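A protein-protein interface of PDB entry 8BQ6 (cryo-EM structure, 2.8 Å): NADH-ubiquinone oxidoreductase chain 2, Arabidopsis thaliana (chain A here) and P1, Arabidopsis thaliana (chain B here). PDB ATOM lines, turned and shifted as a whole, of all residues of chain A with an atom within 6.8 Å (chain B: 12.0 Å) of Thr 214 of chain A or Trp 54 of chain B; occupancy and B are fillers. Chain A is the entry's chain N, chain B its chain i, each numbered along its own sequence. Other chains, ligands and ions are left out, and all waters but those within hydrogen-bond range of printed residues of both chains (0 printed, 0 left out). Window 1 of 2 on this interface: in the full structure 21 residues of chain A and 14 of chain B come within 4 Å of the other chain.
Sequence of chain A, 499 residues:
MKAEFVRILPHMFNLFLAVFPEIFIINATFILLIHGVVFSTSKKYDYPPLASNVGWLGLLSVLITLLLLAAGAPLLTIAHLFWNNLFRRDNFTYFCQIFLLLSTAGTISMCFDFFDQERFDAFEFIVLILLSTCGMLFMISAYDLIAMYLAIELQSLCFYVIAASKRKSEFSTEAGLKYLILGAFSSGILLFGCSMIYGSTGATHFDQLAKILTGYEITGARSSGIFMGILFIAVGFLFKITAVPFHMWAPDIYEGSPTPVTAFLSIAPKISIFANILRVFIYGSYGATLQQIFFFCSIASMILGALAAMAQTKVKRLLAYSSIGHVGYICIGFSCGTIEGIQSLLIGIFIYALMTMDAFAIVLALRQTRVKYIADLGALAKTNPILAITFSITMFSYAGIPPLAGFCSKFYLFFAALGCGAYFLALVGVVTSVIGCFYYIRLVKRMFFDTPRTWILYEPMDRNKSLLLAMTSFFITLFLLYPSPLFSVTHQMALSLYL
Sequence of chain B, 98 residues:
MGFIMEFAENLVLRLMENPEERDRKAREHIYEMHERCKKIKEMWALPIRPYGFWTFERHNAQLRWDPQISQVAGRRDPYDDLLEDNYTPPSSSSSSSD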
ATOM      1  N   LEU A 209     -10.570   5.461  15.130  1.00  0.00           N
ATOM      2  CA  LEU A 209      -9.770   6.555  14.596  1.00  0.00           C
ATOM      3  C   LEU A 209     -10.476   7.888  14.777  1.00  0.00           C
ATOM      4  O   LEU A 209      -9.834   8.911  15.035  1.00  0.00           O
ATOM      5  CB  LEU A 209      -9.479   6.319  13.118  1.00  0.00           C
ATOM      6  CG  LEU A 209      -8.606   5.125  12.758  1.00  0.00           C
ATOM      7  CD1 LEU A 209      -8.492   5.018  11.251  1.00  0.00           C
ATOM      8  CD2 LEU A 209      -7.249   5.288  13.389  1.00  0.00           C
ATOM      9  N   ALA A 210     -11.800   7.899  14.621  1.00  0.00           N
ATOM     10  CA  ALA A 210     -12.556   9.117  14.872  1.00  0.00           C
ATOM     11  C   ALA A 210     -12.387   9.568  16.316  1.00  0.00           C
ATOM     12  O   ALA A 210     -12.021  10.715  16.580  1.00  0.00           O
ATOM     13  CB  ALA A 210     -14.030   8.895  14.535  1.00  0.00           C
ATOM     14  N   LYS A 211     -12.597   8.661  17.268  1.00  0.00           N
ATOM     15  CA  LYS A 211     -12.512   9.055  18.672  1.00  0.00           C
ATOM     16  C   LYS A 211     -11.109   9.521  19.047  1.00  0.00           C
ATOM     17  O   LYS A 211     -10.951  10.490  19.798  1.00  0.00           O
ATOM     18  CB  LYS A 211     -12.949   7.900  19.562  1.00  0.00           C
ATOM     19  CG  LYS A 211     -14.441   7.768  19.647  1.00  0.00           C
ATOM     20  CD  LYS A 211     -14.820   6.526  20.400  1.00  0.00           C
ATOM     21  CE  LYS A 211     -16.259   6.600  20.848  1.00  0.00           C
ATOM     22  NZ  LYS A 211     -17.193   6.327  19.727  1.00  0.00           N
ATOM     23  N   ILE A 212     -10.080   8.843  18.535  1.00  0.00           N
ATOM     24  CA  ILE A 212      -8.704   9.182  18.893  1.00  0.00           C
ATOM     25  C   ILE A 212      -8.332  10.559  18.356  1.00  0.00           C
ATOM     26  O   ILE A 212      -7.643  11.340  19.024  1.00  0.00           O
ATOM     27  CB  ILE A 212      -7.732   8.108  18.373  1.00  0.00           C
ATOM     28  CG1 ILE A 212      -7.824   6.838  19.203  1.00  0.00           C
ATOM     29  CG2 ILE A 212      -6.305   8.602  18.425  1.00  0.00           C
ATOM     30  CD1 ILE A 212      -7.528   5.592  18.404  1.00  0.00           C
ATOM     31  N   LEU A 213      -8.777  10.879  17.142  1.00  0.00           N
ATOM     32  CA  LEU A 213      -8.239  12.037  16.440  1.00  0.00           C
ATOM     33  C   LEU A 213      -9.076  13.304  16.583  1.00  0.00           C
ATOM     34  O   LEU A 213      -8.572  14.387  16.263  1.00  0.00           O
ATOM     35  CB  LEU A 213      -8.067  11.715  14.956  1.00  0.00           C
ATOM     36  CG  LEU A 213      -7.170  10.579  14.465  1.00  0.00           C
ATOM     37  CD1 LEU A 213      -6.891  10.765  12.988  1.00  0.00           C
ATOM     38  CD2 LEU A 213      -5.873  10.539  15.236  1.00  0.00           C
ATOM     39  N   THR A 214     -10.326  13.219  17.034  1.00  0.00           N
ATOM     40  CA  THR A 214     -11.135  14.423  17.177  1.00  0.00           C
ATOM     41  C   THR A 214     -10.765  15.217  18.421  1.00  0.00           C
ATOM     42  O   THR A 214     -10.410  14.655  19.460  1.00  0.00           O
ATOM     43  CB  THR A 214     -12.625  14.100  17.230  1.00  0.00           C
ATOM     44  OG1 THR A 214     -12.952  13.413  18.449  1.00  0.00           O
ATOM     45  CG2 THR A 214     -13.101  13.337  15.999  1.00  0.00           C
ATOM     46  N   GLY A 215     -10.882  16.540  18.305  1.00  0.00           N
ATOM     47  CA  GLY A 215     -10.599  17.456  19.384  1.00  0.00           C
ATOM     48  C   GLY A 215      -9.169  17.933  19.456  1.00  0.00           C
ATOM     49  O   GLY A 215      -8.865  18.803  20.282  1.00  0.00           O
ATOM     50  N   TYR A 216      -8.284  17.402  18.630  1.00  0.00           N
ATOM     51  CA  TYR A 216      -6.883  17.752  18.810  1.00  0.00           C
ATOM     52  C   TYR A 216      -6.235  18.319  17.560  1.00  0.00           C
ATOM     53  O   TYR A 216      -5.535  19.332  17.653  1.00  0.00           O
ATOM     54  CB  TYR A 216      -6.137  16.507  19.310  1.00  0.00           C
ATOM     55  CG  TYR A 216      -6.501  16.203  20.739  1.00  0.00           C
ATOM     56  CD1 TYR A 216      -7.643  15.470  21.038  1.00  0.00           C
ATOM     57  CD2 TYR A 216      -5.729  16.672  21.791  1.00  0.00           C
ATOM     58  CE1 TYR A 216      -8.000  15.209  22.339  1.00  0.00           C
ATOM     59  CE2 TYR A 216      -6.075  16.408  23.100  1.00  0.00           C
ATOM     60  CZ  TYR A 216      -7.210  15.674  23.368  1.00  0.00           C
ATOM     61  OH  TYR A 216      -7.562  15.406  24.670  1.00  0.00           O
ATOM     62  N   GLU A 217      -6.470  17.660  16.414  1.00  0.00           N
ATOM     63  CA  GLU A 217      -5.824  18.053  15.126  1.00  0.00           C
ATOM     64  C   GLU A 217      -4.342  18.313  15.400  1.00  0.00           C
ATOM     65  O   GLU A 217      -3.669  17.408  15.925  1.00  0.00           O
ATOM     66  CB  GLU A 217      -6.510  19.260  14.466  1.00  0.00           C
ATOM     67  CG  GLU A 217      -7.981  19.442  14.814  1.00  0.00           C
ATOM     68  CD  GLU A 217      -8.941  18.371  14.323  1.00  0.00           C
ATOM     69  OE1 GLU A 217      -9.208  18.326  13.106  1.00  0.00           O
ATOM     70  OE2 GLU A 217      -9.435  17.595  15.164  1.00  0.00           O
ATOM     71  N   TYR A 283     -14.871  12.142   7.966  1.00  0.00           N
ATOM     72  CA  TYR A 283     -15.338  11.443   9.145  1.00  0.00           C
ATOM     73  C   TYR A 283     -14.266  11.330  10.216  1.00  0.00           C
ATOM     74  O   TYR A 283     -14.540  11.637  11.381  1.00  0.00           O
ATOM     75  CB  TYR A 283     -15.809  10.073   8.690  1.00  0.00           C
ATOM     76  CG  TYR A 283     -16.265   9.092   9.718  1.00  0.00           C
ATOM     77  CD1 TYR A 283     -17.512   9.176  10.328  1.00  0.00           C
ATOM     78  CD2 TYR A 283     -15.460   8.016  10.014  1.00  0.00           C
ATOM     79  CE1 TYR A 283     -17.909   8.225  11.245  1.00  0.00           C
ATOM     80  CE2 TYR A 283     -15.842   7.078  10.897  1.00  0.00           C
ATOM     81  CZ  TYR A 283     -17.061   7.176  11.522  1.00  0.00           C
ATOM     82  OH  TYR A 283     -17.404   6.210  12.439  1.00  0.00           O
ATOM     83  N   GLY A 284     -13.043  10.936   9.852  1.00  0.00           N
ATOM     84  CA  GLY A 284     -11.905  11.085  10.710  1.00  0.00           C
ATOM     85  C   GLY A 284     -11.652  12.539  11.037  1.00  0.00           C
ATOM     86  O   GLY A 284     -12.479  13.423  10.773  1.00  0.00           O
ATOM     87  N   SER A 285     -10.519  12.878  11.663  1.00  0.00           N
ATOM     88  CA  SER A 285     -10.404  14.325  12.022  1.00  0.00           C
ATOM     89  C   SER A 285      -8.979  14.880  12.099  1.00  0.00           C
ATOM     90  O   SER A 285      -8.536  15.206  13.220  1.00  0.00           O
ATOM     91  CB  SER A 285     -11.151  14.636  13.302  1.00  0.00           C
ATOM     92  OG  SER A 285     -12.545  14.439  13.136  1.00  0.00           O
ATOM     93  N   TYR A 286      -8.294  15.031  10.962  1.00  0.00           N
ATOM     94  CA  TYR A 286      -6.992  15.754  11.052  1.00  0.00           C
ATOM     95  C   TYR A 286      -7.253  17.219  10.665  1.00  0.00           C
ATOM     96  O   TYR A 286      -6.571  18.094  11.235  1.00  0.00           O
ATOM     97  CB  TYR A 286      -5.823  15.008  10.409  1.00  0.00           C
ATOM     98  CG  TYR A 286      -4.595  15.879  10.477  1.00  0.00           C
ATOM     99  CD1 TYR A 286      -3.905  16.001  11.672  1.00  0.00           C
ATOM    100  CD2 TYR A 286      -4.162  16.632   9.400  1.00  0.00           C
ATOM    101  CE1 TYR A 286      -2.790  16.812  11.793  1.00  0.00           C
ATOM    102  CE2 TYR A 286      -3.047  17.450   9.504  1.00  0.00           C
ATOM    103  CZ  TYR A 286      -2.360  17.540  10.701  1.00  0.00           C
ATOM    104  OH  TYR A 286      -1.255  18.329  10.816  1.00  0.00           O
ATOM    105  N   PRO B  47     -23.469  23.294  11.115  1.00  0.00           N
ATOM    106  CA  PRO B  47     -22.131  22.691  11.131  1.00  0.00           C
ATOM    107  C   PRO B  47     -22.099  21.391  10.347  1.00  0.00           C
ATOM    108  O   PRO B  47     -22.975  20.533  10.486  1.00  0.00           O
ATOM    109  CB  PRO B  47     -21.868  22.453  12.621  1.00  0.00           C
ATOM    110  CG  PRO B  47     -23.226  22.330  13.217  1.00  0.00           C
ATOM    111  CD  PRO B  47     -24.078  23.309  12.455  1.00  0.00           C
ATOM    112  N   ILE B  48     -21.073  21.254   9.513  1.00  0.00           N
ATOM    113  CA  ILE B  48     -20.864  19.991   8.824  1.00  0.00           C
ATOM    114  C   ILE B  48     -20.588  18.882   9.828  1.00  0.00           C
ATOM    115  O   ILE B  48     -21.101  17.766   9.687  1.00  0.00           O
ATOM    116  CB  ILE B  48     -19.724  20.136   7.805  1.00  0.00           C
ATOM    117  CG1 ILE B  48     -19.373  18.776   7.229  1.00  0.00           C
ATOM    118  CG2 ILE B  48     -18.506  20.777   8.456  1.00  0.00           C
ATOM    119  CD1 ILE B  48     -18.217  18.782   6.284  1.00  0.00           C
ATOM    120  N   ARG B  49     -19.791  19.173  10.854  1.00  0.00           N
ATOM    121  CA  ARG B  49     -19.502  18.276  11.960  1.00  0.00           C
ATOM    122  C   ARG B  49     -20.361  18.699  13.140  1.00  0.00           C
ATOM    123  O   ARG B  49     -20.099  19.751  13.744  1.00  0.00           O
ATOM    124  CB  ARG B  49     -18.017  18.344  12.321  1.00  0.00           C
ATOM    125  CG  ARG B  49     -17.637  17.559  13.558  1.00  0.00           C
ATOM    126  CD  ARG B  49     -16.596  18.290  14.398  1.00  0.00           C
ATOM    127  NE  ARG B  49     -15.568  18.939  13.593  1.00  0.00           N
ATOM    128  CZ  ARG B  49     -15.266  20.228  13.661  1.00  0.00           C
ATOM    129  NH1 ARG B  49     -15.906  21.046  14.483  1.00  0.00           N
ATOM    130  NH2 ARG B  49     -14.295  20.708  12.889  1.00  0.00           N
ATOM    131  N   PRO B  50     -21.417  17.956  13.579  1.00  0.00           N
ATOM    132  CA  PRO B  50     -22.266  18.473  14.670  1.00  0.00           C
ATOM    133  C   PRO B  50     -21.602  18.454  16.058  1.00  0.00           C
ATOM    134  O   PRO B  50     -20.444  18.075  16.174  1.00  0.00           O
ATOM    135  CB  PRO B  50     -23.486  17.541  14.671  1.00  0.00           C
ATOM    136  CG  PRO B  50     -22.933  16.229  14.181  1.00  0.00           C
ATOM    137  CD  PRO B  50     -21.910  16.620  13.139  1.00  0.00           C
ATOM    138  N   TYR B  51     -22.355  18.858  17.082  1.00  0.00           N
ATOM    139  CA  TYR B  51     -21.789  18.910  18.450  1.00  0.00           C
ATOM    140  C   TYR B  51     -21.648  17.495  18.991  1.00  0.00           C
ATOM    141  O   TYR B  51     -22.661  16.924  19.454  1.00  0.00           O
ATOM    142  CB  TYR B  51     -22.648  19.738  19.406  1.00  0.00           C
ATOM    143  CG  TYR B  51     -21.831  20.328  20.524  1.00  0.00           C
ATOM    144  CD1 TYR B  51     -20.612  20.926  20.255  1.00  0.00           C
ATOM    145  CD2 TYR B  51     -22.249  20.261  21.842  1.00  0.00           C
ATOM    146  CE1 TYR B  51     -19.842  21.479  21.263  1.00  0.00           C
ATOM    147  CE2 TYR B  51     -21.493  20.813  22.865  1.00  0.00           C
ATOM    148  CZ  TYR B  51     -20.286  21.421  22.571  1.00  0.00           C
ATOM    149  OH  TYR B  51     -19.524  21.974  23.553  1.00  0.00           O
ATOM    150  N   GLY B  52     -20.430  16.959  18.933  1.00  0.00           N
ATOM    151  CA  GLY B  52     -20.183  15.607  19.454  1.00  0.00           C
ATOM    152  C   GLY B  52     -20.796  14.548  18.568  1.00  0.00           C
ATOM    153  O   GLY B  52     -21.783  13.939  18.995  1.00  0.00           O
ATOM    154  N   PHE B  53     -20.258  14.347  17.363  1.00  0.00           N
ATOM    155  CA  PHE B  53     -20.785  13.220  16.548  1.00  0.00           C
ATOM    156  C   PHE B  53     -20.500  11.938  17.338  1.00  0.00           C
ATOM    157  O   PHE B  53     -21.427  11.150  17.479  1.00  0.00           O
ATOM    158  CB  PHE B  53     -20.269  13.256  15.105  1.00  0.00           C
ATOM    159  CG  PHE B  53     -18.836  12.852  14.872  1.00  0.00           C
ATOM    160  CD1 PHE B  53     -17.835  13.805  14.827  1.00  0.00           C
ATOM    161  CD2 PHE B  53     -18.497  11.527  14.647  1.00  0.00           C
ATOM    162  CE1 PHE B  53     -16.520  13.440  14.595  1.00  0.00           C
ATOM    163  CE2 PHE B  53     -17.179  11.161  14.428  1.00  0.00           C
ATOM    164  CZ  PHE B  53     -16.195  12.119  14.398  1.00  0.00           C
ATOM    165  N   TRP B  54     -19.311  11.814  17.939  1.00  0.00           N
ATOM    166  CA  TRP B  54     -18.925  10.627  18.756  1.00  0.00           C
ATOM    167  C   TRP B  54     -20.051  10.222  19.722  1.00  0.00           C
ATOM    168  O   TRP B  54     -20.218   9.004  19.940  1.00  0.00           O
ATOM    169  CB  TRP B  54     -17.591  10.897  19.476  1.00  0.00           C
ATOM    170  CG  TRP B  54     -17.468  12.228  20.153  1.00  0.00           C
ATOM    171  CD1 TRP B  54     -17.768  12.519  21.450  1.00  0.00           C
ATOM    172  CD2 TRP B  54     -16.972  13.452  19.580  1.00  0.00           C
ATOM    173  NE1 TRP B  54     -17.506  13.832  21.724  1.00  0.00           N
ATOM    174  CE2 TRP B  54     -17.019  14.431  20.595  1.00  0.00           C
ATOM    175  CE3 TRP B  54     -16.507  13.819  18.314  1.00  0.00           C
ATOM    176  CZ2 TRP B  54     -16.624  15.749  20.376  1.00  0.00           C
ATOM    177  CZ3 TRP B  54     -16.115  15.120  18.098  1.00  0.00           C
ATOM    178  CH2 TRP B  54     -16.168  16.070  19.118  1.00  0.00           C
ATOM    179  N   THR B  55     -20.812  11.189  20.253  1.00  0.00           N
ATOM    180  CA  THR B  55     -21.921  10.921  21.212  1.00  0.00           C
ATOM    181  C   THR B  55     -23.029  10.042  20.601  1.00  0.00           C
ATOM    182  O   THR B  55     -23.649   9.302  21.381  1.00  0.00           O
ATOM    183  CB  THR B  55     -22.484  12.257  21.727  1.00  0.00           C
ATOM    184  OG1 THR B  55     -21.412  13.185  21.906  1.00  0.00           O
ATOM    185  CG2 THR B  55     -23.241  12.138  23.032  1.00  0.00           C
ATOM    186  N   PHE B  56     -23.257  10.068  19.278  1.00  0.00           N
ATOM    187  CA  PHE B  56     -24.403   9.345  18.642  1.00  0.00           C
ATOM    188  C   PHE B  56     -24.287   7.824  18.765  1.00  0.00           C
ATOM    189  O   PHE B  56     -23.146   7.320  18.805  1.00  0.00           O
ATOM    190  CB  PHE B  56     -24.558   9.725  17.168  1.00  0.00           C
ATOM    191  CG  PHE B  56     -24.699  11.197  16.879  1.00  0.00           C
ATOM    192  CD1 PHE B  56     -25.199  12.076  17.829  1.00  0.00           C
ATOM    193  CD2 PHE B  56     -24.343  11.705  15.640  1.00  0.00           C
ATOM    194  CE1 PHE B  56     -25.318  13.429  17.554  1.00  0.00           C
ATOM    195  CE2 PHE B  56     -24.470  13.057  15.362  1.00  0.00           C
ATOM    196  CZ  PHE B  56     -24.956  13.915  16.320  1.00  0.00           C
ATOM    197  N   GLU B  57     -25.422   7.109  18.726  1.00  0.00           N
ATOM    198  CA  GLU B  57     -25.418   5.670  18.969  1.00  0.00           C
ATOM    199  C   GLU B  57     -24.824   4.881  17.808  1.00  0.00           C
ATOM    200  O   GLU B  57     -24.328   3.767  18.011  1.00  0.00           O
ATOM    201  CB  GLU B  57     -26.841   5.189  19.255  1.00  0.00           C
ATOM    202  CG  GLU B  57     -26.912   3.946  20.128  1.00  0.00           C
ATOM    203  CD  GLU B  57     -28.060   3.029  19.746  1.00  0.00           C
ATOM    204  OE1 GLU B  57     -27.931   2.311  18.733  1.00  0.00           O
ATOM    205  OE2 GLU B  57     -29.084   3.019  20.461  1.00  0.00           O
ATOM    206  N   ARG B  58     -24.875   5.419  16.589  1.00  0.00           N
ATOM    207  CA  ARG B  58     -24.199   4.741  15.489  1.00  0.00           C
ATOM    208  C   ARG B  58     -22.697   4.673  15.731  1.00  0.00           C
ATOM    209  O   ARG B  58     -22.038   3.717  15.307  1.00  0.00           O
ATOM    210  CB  ARG B  58     -24.494   5.443  14.161  1.00  0.00           C
ATOM    211  CG  ARG B  58     -23.602   4.998  13.001  1.00  0.00           C
ATOM    212  CD  ARG B  58     -23.968   3.599  12.500  1.00  0.00           C
ATOM    213  NE  ARG B  58     -23.275   2.537  13.224  1.00  0.00           N
ATOM    214  CZ  ARG B  58     -23.571   1.247  13.133  1.00  0.00           C
ATOM    215  NH1 ARG B  58     -24.549   0.814  12.358  1.00  0.00           N
ATOM    216  NH2 ARG B  58     -22.853   0.366  13.825  1.00  0.00           N
ATOM    217  N   HIS B  59     -22.152   5.654  16.446  1.00  0.00           N
ATOM    218  CA  HIS B  59     -20.720   5.771  16.673  1.00  0.00           C
ATOM    219  C   HIS B  59     -20.243   5.027  17.911  1.00  0.00           C
ATOM    220  O   HIS B  59     -19.047   5.071  18.216  1.00  0.00           O
ATOM    221  CB  HIS B  59     -20.344   7.247  16.795  1.00  0.00           C
ATOM    222  CG  HIS B  59     -20.674   8.046  15.576  1.00  0.00           C
ATOM    223  ND1 HIS B  59     -21.522   9.131  15.602  1.00  0.00           N
ATOM    224  CD2 HIS B  59     -20.284   7.904  14.290  1.00  0.00           C
ATOM    225  CE1 HIS B  59     -21.633   9.630  14.383  1.00  0.00           C
ATOM    226  NE2 HIS B  59     -20.889   8.903  13.568  1.00  0.00           N
ATOM    227  N   ASN B  60     -21.138   4.354  18.629  1.00  0.00           N
ATOM    228  CA  ASN B  60     -20.780   3.602  19.829  1.00  0.00           C
ATOM    229  C   ASN B  60     -21.032   2.113  19.658  1.00  0.00           C
ATOM    230  O   ASN B  60     -21.531   1.449  20.569  1.00  0.00           O
ATOM    231  CB  ASN B  60     -21.543   4.146  21.031  1.00  0.00           C
ATOM    232  CG  ASN B  60     -21.290   5.618  21.252  1.00  0.00           C
ATOM    233  OD1 ASN B  60     -20.143   6.066  21.256  1.00  0.00           O
ATOM    234  ND2 ASN B  60     -22.361   6.387  21.409  1.00  0.00           N
ATOM    235  N   ALA B  61     -20.697   1.564  18.491  1.00  0.00           N
ATOM    236  CA  ALA B  61     -20.939   0.146  18.251  1.00  0.00           C
ATOM    237  C   ALA B  61     -20.040  -0.731  19.119  1.00  0.00           C
ATOM    238  O   ALA B  61     -20.490  -1.750  19.655  1.00  0.00           O
ATOM    239  CB  ALA B  61     -20.745  -0.173  16.770  1.00  0.00           C
ATOM    240  N   GLN B  62     -18.763  -0.365  19.238  1.00  0.00           N
ATOM    241  CA  GLN B  62     -17.795  -1.178  20.025  1.00  0.00           C
ATOM    242  C   GLN B  62     -18.240  -1.279  21.490  1.00  0.00           C
ATOM    243  O   GLN B  62     -18.131  -2.368  22.057  1.00  0.00           O
ATOM    244  CB  GLN B  62     -16.403  -0.559  19.900  1.00  0.00           C
ATOM    245  CG  GLN B  62     -15.373  -1.164  20.844  1.00  0.00           C
ATOM    246  CD  GLN B  62     -13.948  -0.877  20.445  1.00  0.00           C
ATOM    247  OE1 GLN B  62     -13.636   0.173  19.892  1.00  0.00           O
ATOM    248  NE2 GLN B  62     -13.063  -1.814  20.737  1.00  0.00           N
ATOM    249  N   LEU B  63     -18.763  -0.194  22.065  1.00  0.00           N
ATOM    250  CA  LEU B  63     -19.132  -0.188  23.476  1.00  0.00           C
ATOM    251  C   LEU B  63     -20.275  -1.146  23.789  1.00  0.00           C
ATOM    252  O   LEU B  63     -20.456  -1.514  24.954  1.00  0.00           O
ATOM    253  CB  LEU B  63     -19.513   1.224  23.905  1.00  0.00           C
ATOM    254  CG  LEU B  63     -18.317   2.118  24.222  1.00  0.00           C
ATOM    255  CD1 LEU B  63     -18.743   3.568  24.323  1.00  0.00           C
ATOM    256  CD2 LEU B  63     -17.636   1.645  25.469  1.00  0.00           C
ATOM    257  N   ARG B  64     -21.052  -1.549  22.788  1.00  0.00           N
ATOM    258  CA  ARG B  64     -22.139  -2.487  23.017  1.00  0.00           C
ATOM    259  C   ARG B  64     -21.833  -3.889  22.520  1.00  0.00           C
ATOM    260  O   ARG B  64     -22.437  -4.849  23.009  1.00  0.00           O
ATOM    261  CB  ARG B  64     -23.424  -1.979  22.355  1.00  0.00           C
ATOM    262  CG  ARG B  64     -23.541  -0.470  22.378  1.00  0.00           C
ATOM    263  CD  ARG B  64     -24.992  -0.029  22.410  1.00  0.00           C
ATOM    264  NE  ARG B  64     -25.708  -0.346  21.180  1.00  0.00           N
ATOM    265  CZ  ARG B  64     -25.578   0.325  20.043  1.00  0.00           C
ATOM    266  NH1 ARG B  64     -24.763   1.363  19.942  1.00  0.00           N
ATOM    267  NH2 ARG B  64     -26.288  -0.051  18.983  1.00  0.00           N
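The side-chain amide oxygen of Asn 60 of chain B lies within hydrogen-bond range of the side-chain amino group of Lys 211 of chain A, at 3.3 Å. The side-chain amino group (NZ) of Lys 211 of chain A lies within hydrogen-bond range of the backbone carbonyl oxygen (O) of His 59 of chain B (2.7 Å).
OG1 of Thr 214 of chain A lies close to O of Ala 210 of chain A (3.4 Å). O of Thr 55 of chain B lies within hydrogen-bond range of ND2 of Asn 60 of chain B. O of Phe 56 of chain B sits at hydrogen-bond distance from ND2 of Asn 60 of chain B. The side-chain amide oxygen (OD1) of Asn 60 of chain B sits close to the backbone carbonyl oxygen (O) of Trp 54 of chain B. The guanidinium group of Arg 64 of chain B lies within hydrogen-bond range of the backbone carbonyl oxygen of Asn 60 of chain B (3.3 Å). The backbone carbonyl oxygen of Phe 53 of chain B lies within hydrogen-bond range of a ring nitrogen (ND1) of His 59 of chain B, 2.8 Å away.
Phe 53 of chain B touches Ala 210 of chain A. CG2 of Thr 214 of chain A touches CZ of Phe 53 of chain B (3.7 Å). OG1 of Thr 214 of chain A touches CE3 of Trp 54 of chain B, at 3.6 Å. Tyr 283 of chain A touches Phe 53 of chain B (O to CZ, 3.5 Å). CD2 of His 59 of chain B touches OH of Tyr 283 of chain A (3.8 Å).
Thr 214 of chain A touches just these residues of chain B: Phe 53 (3.7 Å) and Trp 54 (3.6 Å). Of the printed residues of chain A, Trp 54 of chain B touches Thr 214. Lys 211 of chain A touches just these residues of chain B: His 59 (2.7 Å) and Asn 60 (3.3 Å). No residue of chain B comes within 4 Å of Leu 213 of chain A. No residue of chain B comes within 4 Å of Gly 215 of chain A. No residue of chain B comes within 4 Å of Glu 217 of chain A. No residue of chain B comes within 4 Å of Gly 284 of chain A. No residue of chain B comes within 4 Å of Ser 285 of chain A. Printed residues of chain A within 4 Å of Asn 60 of chain B: Lys 211. Printed residues of chain B within 4 Å of Tyr 283 of chain A: Phe 53 and His 59. The nearest residue of chain B that does not touch Thr 214 of chain A is Arg 49 of chain B (6.3 Å). The nearest printed residue of chain B that does not touch Tyr 283 of chain A is Arg 58 of chain B (6.0 Å).
Of the 13 printed residues of chain A, 4 touch a printed residue of chain B. Printed residues of chain A that touch a printed residue of chain B: Ala 210, Lys 211, Thr 214 and Tyr 283. Of the 18 printed residues of chain B, 4 touch a printed residue of chain A. Printed residues of chain B that touch a printed residue of chain A: Phe 53, Trp 54, His 59 and Asn 60. Among the printed residues, 7 pairs touch across the chains.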
